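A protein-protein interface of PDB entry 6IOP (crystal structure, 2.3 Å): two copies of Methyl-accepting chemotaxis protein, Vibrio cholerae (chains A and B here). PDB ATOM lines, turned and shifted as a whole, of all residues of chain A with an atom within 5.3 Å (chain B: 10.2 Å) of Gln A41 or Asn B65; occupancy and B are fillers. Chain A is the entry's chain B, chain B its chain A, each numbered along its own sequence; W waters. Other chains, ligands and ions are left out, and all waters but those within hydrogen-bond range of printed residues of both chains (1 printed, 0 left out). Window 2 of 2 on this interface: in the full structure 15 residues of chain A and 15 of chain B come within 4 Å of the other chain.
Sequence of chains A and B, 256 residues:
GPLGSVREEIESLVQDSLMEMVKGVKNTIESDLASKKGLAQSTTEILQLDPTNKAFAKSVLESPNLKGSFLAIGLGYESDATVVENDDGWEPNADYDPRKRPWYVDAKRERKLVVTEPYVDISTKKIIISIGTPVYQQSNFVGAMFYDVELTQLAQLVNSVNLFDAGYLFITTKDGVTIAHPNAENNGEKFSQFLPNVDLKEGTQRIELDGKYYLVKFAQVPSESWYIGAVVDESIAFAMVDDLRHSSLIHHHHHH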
ATOM      1  N   LYS A  36      -1.668  -6.531  32.003  1.00  0.00           N
ATOM      2  CA  LYS A  36      -2.323  -7.819  32.075  1.00  0.00           C
ATOM      3  C   LYS A  36      -3.839  -7.695  31.980  1.00  0.00           C
ATOM      4  O   LYS A  36      -4.523  -8.652  31.608  1.00  0.00           O
ATOM      5  CB  LYS A  36      -1.919  -8.537  33.369  1.00  0.00           C
ATOM      6  CG  LYS A  36      -0.442  -8.896  33.377  1.00  0.00           C
ATOM      7  CD  LYS A  36      -0.058  -9.705  34.593  1.00  0.00           C
ATOM      8  CE  LYS A  36       1.386 -10.206  34.439  1.00  0.00           C
ATOM      9  NZ  LYS A  36       1.834 -10.200  33.001  1.00  0.00           N
ATOM     10  N   LYS A  37      -4.358  -6.515  32.305  1.00  0.00           N
ATOM     11  CA  LYS A  37      -5.798  -6.282  32.311  1.00  0.00           C
ATOM     12  C   LYS A  37      -6.345  -6.200  30.897  1.00  0.00           C
ATOM     13  O   LYS A  37      -7.449  -6.682  30.617  1.00  0.00           O
ATOM     14  CB  LYS A  37      -6.151  -5.001  33.095  1.00  0.00           C
ATOM     15  CG  LYS A  37      -6.284  -5.215  34.613  1.00  0.00           C
ATOM     16  CD  LYS A  37      -6.983  -4.044  35.332  1.00  0.00           C
ATOM     17  CE  LYS A  37      -6.034  -2.954  35.763  1.00  0.00           C
ATOM     18  NZ  LYS A  37      -6.716  -2.004  36.712  1.00  0.00           N
ATOM     19  N   GLY A  38      -5.573  -5.597  30.004  1.00  0.00           N
ATOM     20  CA  GLY A  38      -6.000  -5.459  28.623  1.00  0.00           C
ATOM     21  C   GLY A  38      -5.954  -6.814  27.934  1.00  0.00           C
ATOM     22  O   GLY A  38      -6.823  -7.152  27.133  1.00  0.00           O
ATOM     23  N   LEU A  39      -4.929  -7.588  28.261  1.00  0.00           N
ATOM     24  CA  LEU A  39      -4.778  -8.933  27.743  1.00  0.00           C
ATOM     25  C   LEU A  39      -5.935  -9.819  28.223  1.00  0.00           C
ATOM     26  O   LEU A  39      -6.519 -10.583  27.449  1.00  0.00           O
ATOM     27  CB  LEU A  39      -3.429  -9.510  28.180  1.00  0.00           C
ATOM     28  CG  LEU A  39      -2.945 -10.816  27.567  1.00  0.00           C
ATOM     29  CD1 LEU A  39      -3.086 -10.780  26.049  1.00  0.00           C
ATOM     30  CD2 LEU A  39      -1.499 -11.075  27.970  1.00  0.00           C
ATOM     31  N   ALA A  40      -6.266  -9.700  29.502  1.00  0.00           N
ATOM     32  CA  ALA A  40      -7.335 -10.500  30.079  1.00  0.00           C
ATOM     33  C   ALA A  40      -8.686 -10.116  29.465  1.00  0.00           C
ATOM     34  O   ALA A  40      -9.492 -10.976  29.164  1.00  0.00           O
ATOM     35  CB  ALA A  40      -7.362 -10.348  31.607  1.00  0.00           C
ATOM     36  N   GLN A  41      -8.898  -8.822  29.258  1.00  0.00           N
ATOM     37  CA  GLN A  41     -10.122  -8.311  28.665  1.00  0.00           C
ATOM     38  C   GLN A  41     -10.327  -8.835  27.237  1.00  0.00           C
ATOM     39  O   GLN A  41     -11.438  -9.264  26.889  1.00  0.00           O
ATOM     40  CB  GLN A  41     -10.111  -6.779  28.669  1.00  0.00           C
ATOM     41  CG  GLN A  41     -11.388  -6.112  28.154  1.00  0.00           C
ATOM     42  CD  GLN A  41     -12.576  -6.351  29.065  1.00  0.00           C
ATOM     43  OE1 GLN A  41     -12.434  -6.389  30.287  1.00  0.00           O
ATOM     44  NE2 GLN A  41     -13.758  -6.529  28.471  1.00  0.00           N
ATOM     45  N   SER A  42      -9.266  -8.801  26.424  1.00  0.00           N
ATOM     46  CA  SER A  42      -9.356  -9.225  25.027  1.00  0.00           C
ATOM     47  C   SER A  42      -9.580 -10.722  24.917  1.00  0.00           C
ATOM     48  O   SER A  42     -10.416 -11.170  24.148  1.00  0.00           O
ATOM     49  CB  SER A  42      -8.101  -8.831  24.252  1.00  0.00           C
ATOM     50  OG  SER A  42      -8.237  -7.534  23.695  1.00  0.00           O
ATOM     51  N   THR A  43      -8.830 -11.479  25.705  1.00  0.00           N
ATOM     52  CA  THR A  43      -8.980 -12.908  25.770  1.00  0.00           C
ATOM     53  C   THR A  43     -10.425 -13.290  26.094  1.00  0.00           C
ATOM     54  O   THR A  43     -10.977 -14.226  25.515  1.00  0.00           O
ATOM     55  CB  THR A  43      -8.059 -13.506  26.831  1.00  0.00           C
ATOM     56  OG1 THR A  43      -6.714 -13.045  26.622  1.00  0.00           O
ATOM     57  CG2 THR A  43      -8.121 -15.034  26.785  1.00  0.00           C
ATOM     58  N   THR A  44     -11.014 -12.561  27.041  1.00  0.00           N
ATOM     59  CA  THR A  44     -12.404 -12.756  27.421  1.00  0.00           C
ATOM     60  C   THR A  44     -13.358 -12.435  26.273  1.00  0.00           C
ATOM     61  O   THR A  44     -14.302 -13.170  26.037  1.00  0.00           O
ATOM     62  CB  THR A  44     -12.778 -11.900  28.650  1.00  0.00           C
ATOM     63  OG1 THR A  44     -11.986 -12.297  29.774  1.00  0.00           O
ATOM     64  CG2 THR A  44     -14.249 -12.076  28.997  1.00  0.00           C
ATOM     65  N   GLU A  45     -13.119 -11.340  25.560  1.00  0.00           N
ATOM     66  CA  GLU A  45     -13.973 -11.006  24.434  1.00  0.00           C
ATOM     67  C   GLU A  45     -13.823 -12.019  23.297  1.00  0.00           C
ATOM     68  O   GLU A  45     -14.781 -12.298  22.590  1.00  0.00           O
ATOM     69  CB  GLU A  45     -13.677  -9.602  23.943  1.00  0.00           C
ATOM     70  CG  GLU A  45     -14.132  -8.540  24.924  1.00  0.00           C
ATOM     71  CD  GLU A  45     -13.630  -7.156  24.557  1.00  0.00           C
ATOM     72  OE1 GLU A  45     -12.897  -7.030  23.545  1.00  0.00           O
ATOM     73  OE2 GLU A  45     -13.970  -6.192  25.276  1.00  0.00           O
ATOM     74  N   ILE A  46     -12.635 -12.594  23.138  1.00  0.00           N
ATOM     75  CA  ILE A  46     -12.444 -13.596  22.102  1.00  0.00           C
ATOM     76  C   ILE A  46     -13.191 -14.889  22.459  1.00  0.00           C
ATOM     77  O   ILE A  46     -13.873 -15.462  21.617  1.00  0.00           O
ATOM     78  CB  ILE A  46     -10.951 -13.875  21.860  1.00  0.00           C
ATOM     79  CG1 ILE A  46     -10.294 -12.629  21.265  1.00  0.00           C
ATOM     80  CG2 ILE A  46     -10.772 -15.041  20.883  1.00  0.00           C
ATOM     81  CD1 ILE A  46      -8.830 -12.788  20.996  1.00  0.00           C
ATOM     82  N   LEU A 113     -14.699  -6.586  34.505  1.00  0.00           N
ATOM     83  CA  LEU A 113     -13.373  -7.033  34.900  1.00  0.00           C
ATOM     84  C   LEU A 113     -13.098  -6.530  36.317  1.00  0.00           C
ATOM     85  O   LEU A 113     -13.272  -5.350  36.616  1.00  0.00           O
ATOM     86  CB  LEU A 113     -12.298  -6.542  33.924  1.00  0.00           C
ATOM     87  CG  LEU A 113     -10.869  -6.974  34.274  1.00  0.00           C
ATOM     88  CD1 LEU A 113     -10.074  -7.218  33.007  1.00  0.00           C
ATOM     89  CD2 LEU A 113     -10.150  -5.950  35.186  1.00  0.00           C
ATOM     90  N   THR A 133     -13.046 -12.047  35.185  1.00  0.00           N
ATOM     91  CA  THR A 133     -13.872 -11.468  34.130  1.00  0.00           C
ATOM     92  C   THR A 133     -15.171 -12.251  33.980  1.00  0.00           C
ATOM     93  O   THR A 133     -15.164 -13.480  34.021  1.00  0.00           O
ATOM     94  CB  THR A 133     -13.128 -11.433  32.764  1.00  0.00           C
ATOM     95  OG1 THR A 133     -12.786 -12.766  32.363  1.00  0.00           O
ATOM     96  CG2 THR A 133     -11.850 -10.602  32.861  1.00  0.00           C
ATOM     97  N   SER B  35       3.071  -3.452  26.427  1.00  0.00           N
ATOM     98  CA  SER B  35       1.756  -4.028  26.636  1.00  0.00           C
ATOM     99  C   SER B  35       1.032  -4.322  25.318  1.00  0.00           C
ATOM    100  O   SER B  35       0.337  -5.319  25.198  1.00  0.00           O
ATOM    101  CB  SER B  35       0.924  -3.086  27.506  1.00  0.00           C
ATOM    102  OG  SER B  35      -0.448  -3.266  27.257  1.00  0.00           O
ATOM    103  N   LYS B  36       1.201  -3.447  24.335  1.00  0.00           N
ATOM    104  CA  LYS B  36       0.631  -3.668  23.027  1.00  0.00           C
ATOM    105  C   LYS B  36       1.288  -4.818  22.268  1.00  0.00           C
ATOM    106  O   LYS B  36       0.615  -5.490  21.494  1.00  0.00           O
ATOM    107  CB  LYS B  36       0.709  -2.390  22.198  1.00  0.00           C
ATOM    108  CG  LYS B  36      -0.450  -1.435  22.503  1.00  0.00           C
ATOM    109  CD  LYS B  36      -0.098  -0.008  22.120  1.00  0.00           C
ATOM    110  CE  LYS B  36      -1.361   0.832  21.929  1.00  0.00           C
ATOM    111  NZ  LYS B  36      -2.362   0.551  23.005  1.00  0.00           N
ATOM    112  N   GLY B  38       2.451  -7.512  23.734  1.00  0.00           N
ATOM    113  CA  GLY B  38       1.894  -8.690  24.372  1.00  0.00           C
ATOM    114  C   GLY B  38       0.541  -9.006  23.754  1.00  0.00           C
ATOM    115  O   GLY B  38       0.235 -10.152  23.406  1.00  0.00           O
ATOM    116  N   LEU B  39      -0.263  -7.965  23.586  1.00  0.00           N
ATOM    117  CA  LEU B  39      -1.591  -8.124  23.030  1.00  0.00           C
ATOM    118  C   LEU B  39      -1.516  -8.621  21.578  1.00  0.00           C
ATOM    119  O   LEU B  39      -2.263  -9.522  21.184  1.00  0.00           O
ATOM    120  CB  LEU B  39      -2.356  -6.807  23.123  1.00  0.00           C
ATOM    121  CG  LEU B  39      -3.846  -6.764  22.793  1.00  0.00           C
ATOM    122  CD1 LEU B  39      -4.588  -7.985  23.337  1.00  0.00           C
ATOM    123  CD2 LEU B  39      -4.441  -5.471  23.353  1.00  0.00           C
ATOM    124  N   ALA B  40      -0.591  -8.051  20.805  1.00  0.00           N
ATOM    125  CA  ALA B  40      -0.441  -8.414  19.401  1.00  0.00           C
ATOM    126  C   ALA B  40       0.103  -9.840  19.240  1.00  0.00           C
ATOM    127  O   ALA B  40      -0.316 -10.558  18.337  1.00  0.00           O
ATOM    128  CB  ALA B  40       0.468  -7.404  18.677  1.00  0.00           C
ATOM    129  N   SER B  42      -0.246 -12.411  21.407  1.00  0.00           N
ATOM    130  CA  SER B  42      -1.355 -13.287  21.784  1.00  0.00           C
ATOM    131  C   SER B  42      -2.456 -13.357  20.731  1.00  0.00           C
ATOM    132  O   SER B  42      -3.005 -14.418  20.481  1.00  0.00           O
ATOM    133  CB  SER B  42      -1.976 -12.842  23.121  1.00  0.00           C
ATOM    134  OG  SER B  42      -1.293 -13.434  24.208  1.00  0.00           O
ATOM    135  N   THR B  43      -2.791 -12.220  20.140  1.00  0.00           N
ATOM    136  CA  THR B  43      -3.785 -12.186  19.078  1.00  0.00           C
ATOM    137  C   THR B  43      -3.321 -12.985  17.859  1.00  0.00           C
ATOM    138  O   THR B  43      -4.116 -13.613  17.170  1.00  0.00           O
ATOM    139  CB  THR B  43      -4.079 -10.749  18.653  1.00  0.00           C
ATOM    140  OG1 THR B  43      -4.618 -10.037  19.772  1.00  0.00           O
ATOM    141  CG2 THR B  43      -5.068 -10.719  17.495  1.00  0.00           C
ATOM    142  N   ILE B  46      -3.509 -16.756  18.669  1.00  0.00           N
ATOM    143  CA  ILE B  46      -4.890 -17.171  18.648  1.00  0.00           C
ATOM    144  C   ILE B  46      -5.382 -17.320  17.198  1.00  0.00           C
ATOM    145  O   ILE B  46      -6.132 -18.249  16.880  1.00  0.00           O
ATOM    146  CB  ILE B  46      -5.756 -16.167  19.456  1.00  0.00           C
ATOM    147  CG1 ILE B  46      -5.731 -16.546  20.945  1.00  0.00           C
ATOM    148  CG2 ILE B  46      -7.202 -16.070  18.908  1.00  0.00           C
ATOM    149  CD1 ILE B  46      -6.094 -15.418  21.887  1.00  0.00           C
ATOM    150  N   SER B  59     -13.902 -11.660  13.174  1.00  0.00           N
ATOM    151  CA  SER B  59     -14.558 -11.616  14.476  1.00  0.00           C
ATOM    152  C   SER B  59     -13.582 -11.178  15.555  1.00  0.00           C
ATOM    153  O   SER B  59     -13.934 -10.408  16.451  1.00  0.00           O
ATOM    154  CB  SER B  59     -15.129 -12.988  14.846  1.00  0.00           C
ATOM    155  OG  SER B  59     -16.080 -13.408  13.887  1.00  0.00           O
ATOM    156  N   VAL B  60     -12.367 -11.706  15.482  1.00  0.00           N
ATOM    157  CA  VAL B  60     -11.366 -11.395  16.481  1.00  0.00           C
ATOM    158  C   VAL B  60     -10.974  -9.923  16.386  1.00  0.00           C
ATOM    159  O   VAL B  60     -11.072  -9.198  17.371  1.00  0.00           O
ATOM    160  CB  VAL B  60     -10.139 -12.305  16.335  1.00  0.00           C
ATOM    161  CG1 VAL B  60      -8.975 -11.813  17.216  1.00  0.00           C
ATOM    162  CG2 VAL B  60     -10.540 -13.745  16.676  1.00  0.00           C
ATOM    163  N   LEU B  61     -10.603  -9.474  15.191  1.00  0.00           N
ATOM    164  CA  LEU B  61     -10.123  -8.106  15.006  1.00  0.00           C
ATOM    165  C   LEU B  61     -11.209  -7.081  15.276  1.00  0.00           C
ATOM    166  O   LEU B  61     -10.915  -5.919  15.540  1.00  0.00           O
ATOM    167  CB  LEU B  61      -9.567  -7.902  13.593  1.00  0.00           C
ATOM    168  CG  LEU B  61      -8.459  -8.832  13.080  1.00  0.00           C
ATOM    169  CD1 LEU B  61      -7.880  -8.310  11.775  1.00  0.00           C
ATOM    170  CD2 LEU B  61      -7.366  -9.007  14.128  1.00  0.00           C
ATOM    171  N   GLU B  62     -12.468  -7.497  15.237  1.00  0.00           N
ATOM    172  CA  GLU B  62     -13.531  -6.542  15.505  1.00  0.00           C
ATOM    173  C   GLU B  62     -13.983  -6.583  16.961  1.00  0.00           C
ATOM    174  O   GLU B  62     -14.814  -5.790  17.345  1.00  0.00           O
ATOM    175  CB  GLU B  62     -14.726  -6.778  14.572  1.00  0.00           C
ATOM    176  CG  GLU B  62     -14.441  -6.497  13.082  1.00  0.00           C
ATOM    177  CD  GLU B  62     -14.354  -5.011  12.753  1.00  0.00           C
ATOM    178  OE1 GLU B  62     -14.842  -4.196  13.549  1.00  0.00           O
ATOM    179  OE2 GLU B  62     -13.806  -4.648  11.691  1.00  0.00           O
ATOM    180  N   SER B  63     -13.457  -7.498  17.771  1.00  0.00           N
ATOM    181  CA  SER B  63     -13.828  -7.500  19.185  1.00  0.00           C
ATOM    182  C   SER B  63     -13.337  -6.187  19.835  1.00  0.00           C
ATOM    183  O   SER B  63     -12.242  -5.727  19.546  1.00  0.00           O
ATOM    184  CB  SER B  63     -13.275  -8.733  19.902  1.00  0.00           C
ATOM    185  OG  SER B  63     -11.888  -8.914  19.676  1.00  0.00           O
ATOM    186  N   PRO B  64     -14.176  -5.568  20.683  1.00  0.00           N
ATOM    187  CA  PRO B  64     -14.044  -4.172  21.145  1.00  0.00           C
ATOM    188  C   PRO B  64     -12.696  -3.758  21.777  1.00  0.00           C
ATOM    189  O   PRO B  64     -12.183  -2.709  21.408  1.00  0.00           O
ATOM    190  CB  PRO B  64     -15.171  -4.043  22.188  1.00  0.00           C
ATOM    191  CG  PRO B  64     -16.140  -5.052  21.835  1.00  0.00           C
ATOM    192  CD  PRO B  64     -15.374  -6.213  21.247  1.00  0.00           C
ATOM    193  N   ASN B  65     -12.148  -4.535  22.702  1.00  0.00           N
ATOM    194  CA  ASN B  65     -10.876  -4.161  23.306  1.00  0.00           C
ATOM    195  C   ASN B  65      -9.759  -4.087  22.274  1.00  0.00           C
ATOM    196  O   ASN B  65      -9.017  -3.115  22.246  1.00  0.00           O
ATOM    197  CB  ASN B  65     -10.479  -5.122  24.433  1.00  0.00           C
ATOM    198  CG  ASN B  65      -9.313  -4.588  25.256  1.00  0.00           C
ATOM    199  OD1 ASN B  65      -8.148  -4.964  25.053  1.00  0.00           O
ATOM    200  ND2 ASN B  65      -9.617  -3.669  26.164  1.00  0.00           N
ATOM    201  N   LEU B  66      -9.658  -5.099  21.416  1.00  0.00           N
ATOM    202  CA  LEU B  66      -8.661  -5.097  20.346  1.00  0.00           C
ATOM    203  C   LEU B  66      -8.840  -3.939  19.397  1.00  0.00           C
ATOM    204  O   LEU B  66      -7.872  -3.275  19.023  1.00  0.00           O
ATOM    205  CB  LEU B  66      -8.718  -6.389  19.541  1.00  0.00           C
ATOM    206  CG  LEU B  66      -7.660  -7.441  19.833  1.00  0.00           C
ATOM    207  CD1 LEU B  66      -7.744  -8.558  18.796  1.00  0.00           C
ATOM    208  CD2 LEU B  66      -6.286  -6.819  19.876  1.00  0.00           C
ATOM    209  N   LYS B  67     -10.079  -3.708  18.983  1.00  0.00           N
ATOM    210  CA  LYS B  67     -10.369  -2.617  18.062  1.00  0.00           C
ATOM    211  C   LYS B  67     -10.128  -1.249  18.728  1.00  0.00           C
ATOM    212  O   LYS B  67      -9.822  -0.264  18.057  1.00  0.00           O
ATOM    213  CB  LYS B  67     -11.807  -2.723  17.556  1.00  0.00           C
ATOM    214  CG  LYS B  67     -12.013  -2.094  16.187  1.00  0.00           C
ATOM    215  CD  LYS B  67     -13.439  -2.286  15.697  1.00  0.00           C
ATOM    216  CE  LYS B  67     -13.681  -1.488  14.432  1.00  0.00           C
ATOM    217  NZ  LYS B  67     -12.923  -0.224  14.514  1.00  0.00           N
ATOM    218  N   GLY B  68     -10.250  -1.198  20.049  1.00  0.00           N
ATOM    219  CA  GLY B  68     -10.011   0.035  20.781  1.00  0.00           C
ATOM    220  C   GLY B  68      -8.543   0.302  21.071  1.00  0.00           C
ATOM    221  O   GLY B  68      -8.138   1.443  21.253  1.00  0.00           O
ATOM    222  N   SER B  69      -7.738  -0.751  21.100  1.00  0.00           N
ATOM    223  CA  SER B  69      -6.371  -0.650  21.587  1.00  0.00           C
ATOM    224  C   SER B  69      -5.368  -0.298  20.496  1.00  0.00           C
ATOM    225  O   SER B  69      -4.201  -0.051  20.785  1.00  0.00           O
ATOM    226  CB  SER B  69      -5.954  -1.958  22.243  1.00  0.00           C
ATOM    227  OG  SER B  69      -6.800  -2.266  23.335  1.00  0.00           O
ATOM    228  N   PHE B  70      -5.830  -0.282  19.254  1.00  0.00           N
ATOM    229  CA  PHE B  70      -4.968  -0.065  18.098  1.00  0.00           C
ATOM    230  C   PHE B  70      -5.637   0.857  17.096  1.00  0.00           C
ATOM    231  O   PHE B  70      -6.853   0.944  17.061  1.00  0.00           O
ATOM    232  CB  PHE B  70      -4.612  -1.398  17.419  1.00  0.00           C
ATOM    233  CG  PHE B  70      -3.674  -2.256  18.228  1.00  0.00           C
ATOM    234  CD1 PHE B  70      -2.307  -1.989  18.243  1.00  0.00           C
ATOM    235  CD2 PHE B  70      -4.155  -3.322  18.978  1.00  0.00           C
ATOM    236  CE1 PHE B  70      -1.431  -2.777  18.996  1.00  0.00           C
ATOM    237  CE2 PHE B  70      -3.293  -4.118  19.727  1.00  0.00           C
ATOM    238  CZ  PHE B  70      -1.923  -3.844  19.730  1.00  0.00           C
ATOM    239  N   LEU B  71      -4.842   1.544  16.287  1.00  0.00           N
ATOM    240  CA  LEU B  71      -5.398   2.371  15.232  1.00  0.00           C
ATOM    241  C   LEU B  71      -6.151   1.474  14.263  1.00  0.00           C
ATOM    242  O   LEU B  71      -7.304   1.748  13.924  1.00  0.00           O
ATOM    243  CB  LEU B  71      -4.302   3.158  14.505  1.00  0.00           C
ATOM    244  CG  LEU B  71      -4.679   4.533  13.939  1.00  0.00           C
ATOM    245  CD1 LEU B  71      -5.277   5.428  15.021  1.00  0.00           C
ATOM    246  CD2 LEU B  71      -3.462   5.213  13.305  1.00  0.00           C
ATOM    247  N   ALA B  72      -5.480   0.401  13.844  1.00  0.00           N
ATOM    248  CA  ALA B  72      -6.030  -0.621  12.954  1.00  0.00           C
ATOM    249  C   ALA B  72      -5.186  -1.904  13.035  1.00  0.00           C
ATOM    250  O   ALA B  72      -4.026  -1.869  13.446  1.00  0.00           O
ATOM    251  CB  ALA B  72      -6.085  -0.113  11.515  1.00  0.00           C
ATOM    252  N   ILE B  73      -5.788  -3.027  12.663  1.00  0.00           N
ATOM    253  CA  ILE B  73      -5.109  -4.317  12.620  1.00  0.00           C
ATOM    254  C   ILE B  73      -5.490  -5.027  11.321  1.00  0.00           C
ATOM    255  O   ILE B  73      -6.641  -4.990  10.905  1.00  0.00           O
ATOM    256  CB  ILE B  73      -5.483  -5.227  13.816  1.00  0.00           C
ATOM    257  CG1 ILE B  73      -5.450  -4.459  15.137  1.00  0.00           C
ATOM    258  CG2 ILE B  73      -4.573  -6.455  13.880  1.00  0.00           C
ATOM    259  CD1 ILE B  73      -6.154  -5.173  16.275  1.00  0.00           C
ATOM    260  N   ASN B  86      -9.699  -4.335  10.194  1.00  0.00           N
ATOM    261  CA  ASN B  86     -10.763  -3.792  11.029  1.00  0.00           C
ATOM    262  C   ASN B  86     -10.857  -2.278  10.911  1.00  0.00           C
ATOM    263  O   ASN B  86     -11.425  -1.614  11.764  1.00  0.00           O
ATOM    264  CB  ASN B  86     -10.559  -4.194  12.498  1.00  0.00           C
ATOM    265  CG  ASN B  86      -9.322  -3.536  13.159  1.00  0.00           C
ATOM    266  OD1 ASN B  86      -8.579  -2.750  12.545  1.00  0.00           O
ATOM    267  ND2 ASN B  86      -9.125  -3.849  14.442  1.00  0.00           N
ATOM    268  N   TYR B 147      -0.212  -4.241  13.282  1.00  0.00           N
ATOM    269  CA  TYR B 147      -0.958  -3.604  14.374  1.00  0.00           C
ATOM    270  C   TYR B 147      -0.519  -2.146  14.467  1.00  0.00           C
ATOM    271  O   TYR B 147       0.595  -1.870  14.914  1.00  0.00           O
ATOM    272  CB  TYR B 147      -0.711  -4.302  15.711  1.00  0.00           C
ATOM    273  CG  TYR B 147      -1.162  -5.751  15.784  1.00  0.00           C
ATOM    274  CD1 TYR B 147      -0.448  -6.759  15.140  1.00  0.00           C
ATOM    275  CD2 TYR B 147      -2.274  -6.117  16.546  1.00  0.00           C
ATOM    276  CE1 TYR B 147      -0.846  -8.081  15.213  1.00  0.00           C
ATOM    277  CE2 TYR B 147      -2.686  -7.447  16.625  1.00  0.00           C
ATOM    278  CZ  TYR B 147      -1.964  -8.422  15.953  1.00  0.00           C
ATOM    279  OH  TYR B 147      -2.355  -9.738  16.030  1.00  0.00           O
ATOM    280  N   ASP B 148      -1.372  -1.216  14.031  1.00  0.00           N
ATOM    281  CA  ASP B 148      -0.997   0.205  14.042  1.00  0.00           C
ATOM    282  C   ASP B 148      -1.188   0.857  15.394  1.00  0.00           C
ATOM    283  O   ASP B 148      -2.272   0.819  15.967  1.00  0.00           O
ATOM    284  CB  ASP B 148      -1.782   0.994  12.990  1.00  0.00           C
ATOM    285  CG  ASP B 148      -1.178   0.856  11.605  1.00  0.00           C
ATOM    286  OD1 ASP B 148      -0.111   0.213  11.489  1.00  0.00           O
ATOM    287  OD2 ASP B 148      -1.757   1.399  10.636  1.00  0.00           O
HETATM  288  O   HOH W   1     -10.882  -7.578  22.110  1.00  0.00           O
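Leu A39 touches Ser B42, and with the chains exchanged Ser A42 touches Leu B39. Ile A46 touches its own counterpart, Ile B46. 7 positions are printed for both chains. Of the 11 pairs that touch across the chains among the printed residues, 3 have their exchanged pair printed and touching as well.
The backbone carbonyl oxygen of Asn B65 sits at hydrogen-bond distance from the side-chain hydroxyl of Ser B69 (2.6 Å). The side-chain hydroxyl (OG) of Ser B63 lies within hydrogen-bond range of the backbone carbonyl oxygen (O) of Val B60. OG1 of Thr A43 sits at hydrogen-bond distance from O of Leu A39, at 2.6 Å. The side-chain amide nitrogen (NE2) of Gln A41 is in hydrogen-bond range of the side-chain carboxylate (OE2) of Glu A45, 3.2 Å away. The backbone carbonyl oxygen of Leu B39 is in hydrogen-bond range of the side-chain hydroxyl of Thr B43 (2.8 Å).
Water W1 lies within hydrogen-bond range of the side-chain carboxylate (OE1) of Glu A45 (2.5 Å), the backbone NH (N) of Leu B66 (2.9 Å), the side-chain hydroxyl (OG) of Ser B63 (3.0 Å), the side-chain hydroxyl (OG) of Ser A42 (3.1 Å) and the backbone NH (N) of Asn B65 (3.3 Å).
Gln A41 touches just one residue of chain B: Asn B65 (3.6 Å). Asn B65 touches just these residues of chain A: Gly A38 (3.3 Å), Gln A41 (3.6 Å), Ser A42 (2.9 Å) and Glu A45 (2.7 Å). Of chain B, only Asn B65 (3.3 Å) comes within 4 Å of Gly A38. No residue of chain B comes within 4 Å of Ala A40. Ser A42 touches three residues of chain B. No residue of chain B comes within 4 Å of Thr A44. Printed residues of chain B within 4 Å of Leu A39: Ser B42 (3.7 Å). Of the printed residues of chain A, Ser B63 touches Glu A45. Of the printed residues of chain A, Leu B66 touches Ser A42 (3.6 Å). Glu B62 touches none of the printed residues of chain A. The nearest residue of chain A that does not touch Asn B65 is Leu A39 (5.2 Å). The nearest printed residue of chain A that does not touch Ser B42 is Thr A43 (5.9 Å).
Among the printed residues, pairs that only touch across the chains: Leu A39 with Ser B42 (3.7 Å), Gln A41 with Asn B65 (3.6 Å), Ser A42 with Leu B39 (3.7 Å), Ser A42 with Leu B66 (3.6 Å), Glu A45 with Ser B63 (3.8 Å), Ile A46 with Ile B46 (3.9 Å) and Ile A46 with Val B60 (3.9 Å).
OD1 of Asn B65 is in hydrogen-bond range of OG of Ser A42 (2.9 Å). The backbone NH (N) of Asn B65 lies within hydrogen-bond range of the side-chain carboxylate (OE1) of Glu A45 (2.7 Å). The side-chain carboxylate (OE1) of Glu A45 sits close to the backbone nitrogen (N) of Pro B64 (3.5 Å). The backbone carbonyl oxygen (O) of Gly A38 sits close to the side-chain amide oxygen (OD1) of Asn B65 (3.3 Å).
Hydrophobic or aromatic side chains of chain A that line the printed part of chain B: Leu A39 and Ile A46. Of the 26 printed residues of chain B, 8 touch a printed residue of chain A. Hydrophobic or aromatic side chains of chain B that line the printed part of chain A: Leu B39, Ile B46, Val B60, Pro B64 and Leu B66. Among the printed residues, 11 pairs touch across the chains. Among the printed residues, no Asp or Glu carboxylate lies within 4 Å of a Lys or Arg side-chain nitrogen of the other chain.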
